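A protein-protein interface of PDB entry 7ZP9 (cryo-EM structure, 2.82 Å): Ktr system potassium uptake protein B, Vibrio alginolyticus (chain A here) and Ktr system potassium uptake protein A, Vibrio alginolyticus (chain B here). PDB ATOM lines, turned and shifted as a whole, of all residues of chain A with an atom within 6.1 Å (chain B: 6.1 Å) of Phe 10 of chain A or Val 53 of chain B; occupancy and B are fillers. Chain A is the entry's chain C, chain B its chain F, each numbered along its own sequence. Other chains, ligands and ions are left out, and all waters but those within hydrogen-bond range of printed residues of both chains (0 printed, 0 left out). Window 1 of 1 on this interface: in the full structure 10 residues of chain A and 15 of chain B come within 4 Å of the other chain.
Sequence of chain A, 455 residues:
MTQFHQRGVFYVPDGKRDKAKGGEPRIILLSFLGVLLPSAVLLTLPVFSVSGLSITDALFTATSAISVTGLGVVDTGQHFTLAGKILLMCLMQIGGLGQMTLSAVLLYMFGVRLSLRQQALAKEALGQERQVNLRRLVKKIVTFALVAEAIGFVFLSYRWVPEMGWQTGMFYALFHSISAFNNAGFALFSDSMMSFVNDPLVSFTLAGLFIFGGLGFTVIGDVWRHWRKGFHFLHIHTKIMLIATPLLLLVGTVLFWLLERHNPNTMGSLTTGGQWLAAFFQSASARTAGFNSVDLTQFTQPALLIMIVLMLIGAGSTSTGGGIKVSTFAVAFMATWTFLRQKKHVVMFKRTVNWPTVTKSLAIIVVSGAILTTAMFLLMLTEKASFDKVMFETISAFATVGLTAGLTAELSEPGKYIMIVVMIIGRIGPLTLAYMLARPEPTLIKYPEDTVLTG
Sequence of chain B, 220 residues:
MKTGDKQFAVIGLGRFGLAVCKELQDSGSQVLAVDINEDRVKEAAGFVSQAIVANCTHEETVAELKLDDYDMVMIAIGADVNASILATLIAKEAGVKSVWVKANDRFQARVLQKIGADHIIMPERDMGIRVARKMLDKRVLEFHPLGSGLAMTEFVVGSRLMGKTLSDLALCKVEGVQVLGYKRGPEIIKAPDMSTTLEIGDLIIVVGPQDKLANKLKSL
Among the printed residues, merely in contact across the chains: Gly 8 of chain A with Thr 61 of chain B (3.7 Å), Gly 8 of chain A with Glu 64 of chain B (3.3 Å), Phe 10 of chain A with Ile 52 of chain B (3.6 Å), Phe 10 of chain A with Val 53 of chain B (3.2 Å), Phe 10 of chain A with Ala 54 of chain B (3.5 Å), Phe 10 of chain A with Glu 64 of chain B (3.6 Å), Tyr 11 of chain A with Glu 38 of chain B (3.0 Å), Tyr 11 of chain A with Ile 52 of chain B (3.6 Å), Val 12 of chain A with Ala 51 of chain B (3.6 Å), Pro 13 of chain A with Val 41 of chain B (3.2 Å), Pro 13 of chain A with Lys 42 of chain B (3.8 Å), Pro 13 of chain A with Ala 51 of chain B (3.3 Å), Pro 13 of chain A with Val 53 of chain B (3.7 Å), Leu 116 of chain A with Ile 36 of chain B (3.4 Å), Leu 116 of chain A with Val 53 of chain B (3.3 Å), Leu 116 of chain A with Ala 54 of chain B (3.8 Å) and Leu 116 of chain A with Asn 55 of chain B (3.7 Å).
O of Tyr 11 of chain A is in hydrogen-bond range of N of Val 53 of chain B (2.9 Å).
OG1 of Thr 61 of chain B is in hydrogen-bond range of N of Val 9 of chain A, 3.2 Å away.
The backbone carbonyl oxygen of Ala 33 of chain B is in hydrogen-bond range of the backbone NH of Ile 52 of chain B, at 2.8 Å.
The backbone NH (N) of Asp 35 of chain B sits at hydrogen-bond distance from the backbone carbonyl oxygen (O) of Ile 52 of chain B (3.3 Å).
The backbone carbonyl oxygen (O) of Asp 35 of chain B sits at hydrogen-bond distance from the backbone NH (N) of Ala 54 of chain B, 3.4 Å away.
The backbone NH of Ile 36 of chain B sits close to the backbone carbonyl oxygen of Ala 54 of chain B (3.4 Å).
Of chain B, only Ile 52, Val 53, Ala 54 and Glu 64 come within 4 Å of Phe 10 of chain A.
Val 53 of chain B touches four residues of chain A.
Of the printed residues of chain B, Pro 13 of chain A touches Val 41 (3.2 Å), Lys 42 (3.8 Å), Ala 51 (3.3 Å) and Val 53 (3.7 Å).
Printed residues of chain A within 4 Å of Thr 61 of chain B: Gly 8 (3.7 Å) and Val 9 (3.2 Å).
Printed residues of chain B within 4 Å of Gly 8 of chain A: Thr 61 and Glu 64.
Of the printed residues of chain A, Ile 52 of chain B touches Phe 10 and Tyr 11.
Ala 33 of chain B touches none of the printed residues of chain A.
Of the 8 printed residues of chain A, 7 touch a printed residue of chain B.
Hydrophobic or aromatic side chains of chain A within 4 Å of the printed part of chain B: Phe 10, Tyr 11, Val 12, Pro 13 and Leu 116.
Printed residues of chain B that touch a printed residue of chain A: Ile 36, Glu 38, Val 41, Lys 42, Ala 51, Ile 52, Val 53, Ala 54, Asn 55, Thr 61 and Glu 64.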
ATOM      1  N   GLY A   8       5.292 -13.247   4.023  1.00  0.00           N
ATOM      2  CA  GLY A   8       6.622 -13.371   3.449  1.00  0.00           C
ATOM      3  C   GLY A   8       6.972 -14.818   3.162  1.00  0.00           C
ATOM      4  O   GLY A   8       6.927 -15.671   4.055  1.00  0.00           O
ATOM      5  N   VAL A   9       7.328 -15.095   1.913  1.00  0.00           N
ATOM      6  CA  VAL A   9       7.736 -16.426   1.480  1.00  0.00           C
ATOM      7  C   VAL A   9       9.249 -16.392   1.309  1.00  0.00           C
ATOM      8  O   VAL A   9       9.760 -15.962   0.272  1.00  0.00           O
ATOM      9  CB  VAL A   9       7.028 -16.843   0.190  1.00  0.00           C
ATOM     10  CG1 VAL A   9       7.294 -18.307  -0.112  1.00  0.00           C
ATOM     11  CG2 VAL A   9       5.538 -16.580   0.301  1.00  0.00           C
ATOM     12  N   PHE A  10       9.974 -16.847   2.328  1.00  0.00           N
ATOM     13  CA  PHE A  10      11.428 -16.852   2.280  1.00  0.00           C
ATOM     14  C   PHE A  10      11.956 -17.886   3.262  1.00  0.00           C
ATOM     15  O   PHE A  10      11.240 -18.344   4.155  1.00  0.00           O
ATOM     16  CB  PHE A  10      12.007 -15.469   2.592  1.00  0.00           C
ATOM     17  CG  PHE A  10      11.628 -14.939   3.945  1.00  0.00           C
ATOM     18  CD1 PHE A  10      10.470 -14.204   4.115  1.00  0.00           C
ATOM     19  CD2 PHE A  10      12.437 -15.167   5.043  1.00  0.00           C
ATOM     20  CE1 PHE A  10      10.121 -13.713   5.354  1.00  0.00           C
ATOM     21  CE2 PHE A  10      12.093 -14.679   6.285  1.00  0.00           C
ATOM     22  CZ  PHE A  10      10.934 -13.950   6.441  1.00  0.00           C
ATOM     23  N   TYR A  11      13.225 -18.246   3.083  1.00  0.00           N
ATOM     24  CA  TYR A  11      13.878 -19.184   3.981  1.00  0.00           C
ATOM     25  C   TYR A  11      15.379 -18.955   3.937  1.00  0.00           C
ATOM     26  O   TYR A  11      15.909 -18.335   3.013  1.00  0.00           O
ATOM     27  CB  TYR A  11      13.559 -20.638   3.617  1.00  0.00           C
ATOM     28  CG  TYR A  11      14.082 -21.071   2.266  1.00  0.00           C
ATOM     29  CD1 TYR A  11      13.404 -20.747   1.102  1.00  0.00           C
ATOM     30  CD2 TYR A  11      15.249 -21.811   2.159  1.00  0.00           C
ATOM     31  CE1 TYR A  11      13.876 -21.144  -0.129  1.00  0.00           C
ATOM     32  CE2 TYR A  11      15.729 -22.212   0.931  1.00  0.00           C
ATOM     33  CZ  TYR A  11      15.036 -21.876  -0.209  1.00  0.00           C
ATOM     34  OH  TYR A  11      15.507 -22.272  -1.436  1.00  0.00           O
ATOM     35  N   VAL A  12      16.060 -19.469   4.955  1.00  0.00           N
ATOM     36  CA  VAL A  12      17.516 -19.424   5.030  1.00  0.00           C
ATOM     37  C   VAL A  12      18.049 -20.767   4.538  1.00  0.00           C
ATOM     38  O   VAL A  12      17.741 -21.800   5.152  1.00  0.00           O
ATOM     39  CB  VAL A  12      17.995 -19.135   6.456  1.00  0.00           C
ATOM     40  CG1 VAL A  12      19.511 -19.131   6.509  1.00  0.00           C
ATOM     41  CG2 VAL A  12      17.433 -17.812   6.943  1.00  0.00           C
ATOM     42  N   PRO A  13      18.821 -20.803   3.454  1.00  0.00           N
ATOM     43  CA  PRO A  13      19.368 -22.080   2.985  1.00  0.00           C
ATOM     44  C   PRO A  13      20.358 -22.654   3.985  1.00  0.00           C
ATOM     45  O   PRO A  13      21.005 -21.927   4.741  1.00  0.00           O
ATOM     46  CB  PRO A  13      20.049 -21.701   1.667  1.00  0.00           C
ATOM     47  CG  PRO A  13      20.432 -20.272   1.882  1.00  0.00           C
ATOM     48  CD  PRO A  13      19.241 -19.692   2.588  1.00  0.00           C
ATOM     49  N   VAL A 112       7.624 -24.016   0.484  1.00  0.00           N
ATOM     50  CA  VAL A 112       8.097 -22.649   0.302  1.00  0.00           C
ATOM     51  C   VAL A 112       9.299 -22.603  -0.636  1.00  0.00           C
ATOM     52  O   VAL A 112       9.447 -21.872  -1.559  1.00  0.00           O
ATOM     53  CB  VAL A 112       8.482 -22.001   1.644  1.00  0.00           C
ATOM     54  CG1 VAL A 112       9.087 -20.624   1.417  1.00  0.00           C
ATOM     55  CG2 VAL A 112       7.271 -21.914   2.560  1.00  0.00           C
ATOM     56  N   LEU A 116       9.672 -20.882  -4.383  1.00  0.00           N
ATOM     57  CA  LEU A 116      10.747 -19.949  -4.695  1.00  0.00           C
ATOM     58  C   LEU A 116      11.608 -20.468  -5.839  1.00  0.00           C
ATOM     59  O   LEU A 116      12.068 -19.686  -6.676  1.00  0.00           O
ATOM     60  CB  LEU A 116      11.586 -19.672  -3.450  1.00  0.00           C
ATOM     61  CG  LEU A 116      10.923 -18.669  -2.503  1.00  0.00           C
ATOM     62  CD1 LEU A 116      11.527 -18.729  -1.118  1.00  0.00           C
ATOM     63  CD2 LEU A 116      11.020 -17.264  -3.071  1.00  0.00           C
ATOM     64  N   ALA B  33      21.885 -10.567   2.370  1.00  0.00           N
ATOM     65  CA  ALA B  33      21.937 -10.959   0.969  1.00  0.00           C
ATOM     66  C   ALA B  33      20.657 -11.701   0.611  1.00  0.00           C
ATOM     67  O   ALA B  33      20.348 -12.736   1.207  1.00  0.00           O
ATOM     68  CB  ALA B  33      23.162 -11.831   0.694  1.00  0.00           C
ATOM     69  N   VAL B  34      19.922 -11.175  -0.362  1.00  0.00           N
ATOM     70  CA  VAL B  34      18.651 -11.742  -0.792  1.00  0.00           C
ATOM     71  C   VAL B  34      18.728 -12.030  -2.284  1.00  0.00           C
ATOM     72  O   VAL B  34      19.167 -11.182  -3.066  1.00  0.00           O
ATOM     73  CB  VAL B  34      17.470 -10.801  -0.484  1.00  0.00           C
ATOM     74  CG1 VAL B  34      16.158 -11.466  -0.850  1.00  0.00           C
ATOM     75  CG2 VAL B  34      17.480 -10.390   0.976  1.00  0.00           C
ATOM     76  N   ASP B  35      18.305 -13.230  -2.674  1.00  0.00           N
ATOM     77  CA  ASP B  35      18.310 -13.618  -4.074  1.00  0.00           C
ATOM     78  C   ASP B  35      17.245 -14.681  -4.288  1.00  0.00           C
ATOM     79  O   ASP B  35      17.058 -15.567  -3.452  1.00  0.00           O
ATOM     80  CB  ASP B  35      19.687 -14.135  -4.500  1.00  0.00           C
ATOM     81  CG  ASP B  35      19.807 -14.320  -5.992  1.00  0.00           C
ATOM     82  OD1 ASP B  35      20.194 -13.354  -6.679  1.00  0.00           O
ATOM     83  OD2 ASP B  35      19.513 -15.425  -6.482  1.00  0.00           O
ATOM     84  N   ILE B  36      16.543 -14.584  -5.420  1.00  0.00           N
ATOM     85  CA  ILE B  36      15.474 -15.533  -5.716  1.00  0.00           C
ATOM     86  C   ILE B  36      16.043 -16.924  -5.970  1.00  0.00           C
ATOM     87  O   ILE B  36      15.387 -17.936  -5.700  1.00  0.00           O
ATOM     88  CB  ILE B  36      14.629 -15.031  -6.903  1.00  0.00           C
ATOM     89  CG1 ILE B  36      13.344 -15.848  -7.041  1.00  0.00           C
ATOM     90  CG2 ILE B  36      15.420 -15.087  -8.199  1.00  0.00           C
ATOM     91  CD1 ILE B  36      12.577 -15.997  -5.759  1.00  0.00           C
ATOM     92  N   ASN B  37      17.267 -16.998  -6.484  1.00  0.00           N
ATOM     93  CA  ASN B  37      17.900 -18.264  -6.825  1.00  0.00           C
ATOM     94  C   ASN B  37      18.614 -18.814  -5.597  1.00  0.00           C
ATOM     95  O   ASN B  37      19.382 -18.097  -4.945  1.00  0.00           O
ATOM     96  CB  ASN B  37      18.866 -18.075  -7.992  1.00  0.00           C
ATOM     97  CG  ASN B  37      19.526 -19.360  -8.416  1.00  0.00           C
ATOM     98  OD1 ASN B  37      20.621 -19.676  -7.965  1.00  0.00           O
ATOM     99  ND2 ASN B  37      18.866 -20.110  -9.286  1.00  0.00           N
ATOM    100  N   GLU B  38      18.365 -20.087  -5.286  1.00  0.00           N
ATOM    101  CA  GLU B  38      18.788 -20.640  -4.004  1.00  0.00           C
ATOM    102  C   GLU B  38      20.289 -20.899  -3.960  1.00  0.00           C
ATOM    103  O   GLU B  38      20.929 -20.669  -2.927  1.00  0.00           O
ATOM    104  CB  GLU B  38      18.006 -21.921  -3.714  1.00  0.00           C
ATOM    105  CG  GLU B  38      18.332 -22.580  -2.387  1.00  0.00           C
ATOM    106  N   VAL B  41      22.281 -17.883  -3.293  1.00  0.00           N
ATOM    107  CA  VAL B  41      22.174 -17.569  -1.872  1.00  0.00           C
ATOM    108  C   VAL B  41      23.127 -18.438  -1.064  1.00  0.00           C
ATOM    109  O   VAL B  41      23.771 -17.962  -0.125  1.00  0.00           O
ATOM    110  CB  VAL B  41      20.721 -17.725  -1.394  1.00  0.00           C
ATOM    111  CG1 VAL B  41      20.644 -17.587   0.113  1.00  0.00           C
ATOM    112  CG2 VAL B  41      19.839 -16.694  -2.057  1.00  0.00           C
ATOM    113  N   LYS B  42      23.233 -19.723  -1.411  1.00  0.00           N
ATOM    114  CA  LYS B  42      24.205 -20.582  -0.739  1.00  0.00           C
ATOM    115  C   LYS B  42      25.628 -20.095  -0.976  1.00  0.00           C
ATOM    116  O   LYS B  42      26.467 -20.136  -0.068  1.00  0.00           O
ATOM    117  CB  LYS B  42      24.055 -22.029  -1.202  1.00  0.00           C
ATOM    118  CG  LYS B  42      22.768 -22.703  -0.771  1.00  0.00           C
ATOM    119  CD  LYS B  42      22.729 -24.145  -1.251  1.00  0.00           C
ATOM    120  CE  LYS B  42      21.436 -24.828  -0.843  1.00  0.00           C
ATOM    121  NZ  LYS B  42      21.372 -26.239  -1.313  1.00  0.00           N
ATOM    122  N   ALA B  51      21.884 -14.759   4.721  1.00  0.00           N
ATOM    123  CA  ALA B  51      21.521 -14.957   3.323  1.00  0.00           C
ATOM    124  C   ALA B  51      20.149 -15.610   3.264  1.00  0.00           C
ATOM    125  O   ALA B  51      19.944 -16.684   3.838  1.00  0.00           O
ATOM    126  CB  ALA B  51      22.562 -15.811   2.601  1.00  0.00           C
ATOM    127  N   ILE B  52      19.215 -14.966   2.566  1.00  0.00           N
ATOM    128  CA  ILE B  52      17.821 -15.384   2.521  1.00  0.00           C
ATOM    129  C   ILE B  52      17.397 -15.557   1.070  1.00  0.00           C
ATOM    130  O   ILE B  52      17.694 -14.708   0.222  1.00  0.00           O
ATOM    131  CB  ILE B  52      16.906 -14.366   3.236  1.00  0.00           C
ATOM    132  CG1 ILE B  52      17.305 -14.229   4.706  1.00  0.00           C
ATOM    133  CG2 ILE B  52      15.449 -14.764   3.108  1.00  0.00           C
ATOM    134  CD1 ILE B  52      16.540 -13.157   5.442  1.00  0.00           C
ATOM    135  N   VAL B  53      16.707 -16.657   0.786  1.00  0.00           N
ATOM    136  CA  VAL B  53      16.115 -16.901  -0.522  1.00  0.00           C
ATOM    137  C   VAL B  53      14.711 -16.313  -0.498  1.00  0.00           C
ATOM    138  O   VAL B  53      13.846 -16.780   0.249  1.00  0.00           O
ATOM    139  CB  VAL B  53      16.081 -18.395  -0.866  1.00  0.00           C
ATOM    140  CG1 VAL B  53      15.709 -18.591  -2.322  1.00  0.00           C
ATOM    141  CG2 VAL B  53      17.414 -19.039  -0.560  1.00  0.00           C
ATOM    142  N   ALA B  54      14.479 -15.288  -1.312  1.00  0.00           N
ATOM    143  CA  ALA B  54      13.188 -14.619  -1.334  1.00  0.00           C
ATOM    144  C   ALA B  54      13.002 -13.922  -2.670  1.00  0.00           C
ATOM    145  O   ALA B  54      13.961 -13.659  -3.397  1.00  0.00           O
ATOM    146  CB  ALA B  54      13.059 -13.612  -0.187  1.00  0.00           C
ATOM    147  N   ASN B  55      11.745 -13.623  -2.983  1.00  0.00           N
ATOM    148  CA  ASN B  55      11.385 -12.845  -4.160  1.00  0.00           C
ATOM    149  C   ASN B  55      11.106 -11.418  -3.713  1.00  0.00           C
ATOM    150  O   ASN B  55      10.174 -11.179  -2.938  1.00  0.00           O
ATOM    151  CB  ASN B  55      10.165 -13.447  -4.857  1.00  0.00           C
ATOM    152  CG  ASN B  55       9.922 -12.854  -6.227  1.00  0.00           C
ATOM    153  OD1 ASN B  55      10.590 -11.909  -6.637  1.00  0.00           O
ATOM    154  ND2 ASN B  55       8.959 -13.414  -6.946  1.00  0.00           N
ATOM    155  N   THR B  61       6.674 -10.060   1.120  1.00  0.00           N
ATOM    156  CA  THR B  61       8.010 -10.565   1.419  1.00  0.00           C
ATOM    157  C   THR B  61       8.960  -9.429   1.781  1.00  0.00           C
ATOM    158  O   THR B  61       9.746  -9.546   2.727  1.00  0.00           O
ATOM    159  CB  THR B  61       8.551 -11.358   0.229  1.00  0.00           C
ATOM    160  OG1 THR B  61       7.800 -12.567   0.079  1.00  0.00           O
ATOM    161  CG2 THR B  61      10.010 -11.707   0.442  1.00  0.00           C
ATOM    162  N   GLU B  64       8.159  -8.332   5.255  1.00  0.00           N
ATOM    163  CA  GLU B  64       8.680  -9.254   6.261  1.00  0.00           C
ATOM    164  C   GLU B  64      10.191  -9.126   6.404  1.00  0.00           C
ATOM    165  O   GLU B  64      10.728  -9.264   7.509  1.00  0.00           O
ATOM    166  CB  GLU B  64       8.288 -10.693   5.922  1.00  0.00           C
ATOM    167  CG  GLU B  64       6.787 -10.924   5.823  1.00  0.00           C
ATOM    168  N   LEU B  65      10.895  -8.870   5.300  1.00  0.00           N
ATOM    169  CA  LEU B  65      12.333  -8.640   5.365  1.00  0.00           C
ATOM    170  C   LEU B  65      12.690  -7.402   6.174  1.00  0.00           C
ATOM    171  O   LEU B  65      13.819  -7.313   6.669  1.00  0.00           O
ATOM    172  CB  LEU B  65      12.910  -8.515   3.955  1.00  0.00           C
ATOM    173  CG  LEU B  65      13.125  -9.820   3.190  1.00  0.00           C
ATOM    174  CD1 LEU B  65      13.679  -9.534   1.807  1.00  0.00           C
ATOM    175  CD2 LEU B  65      14.052 -10.741   3.963  1.00  0.00           C
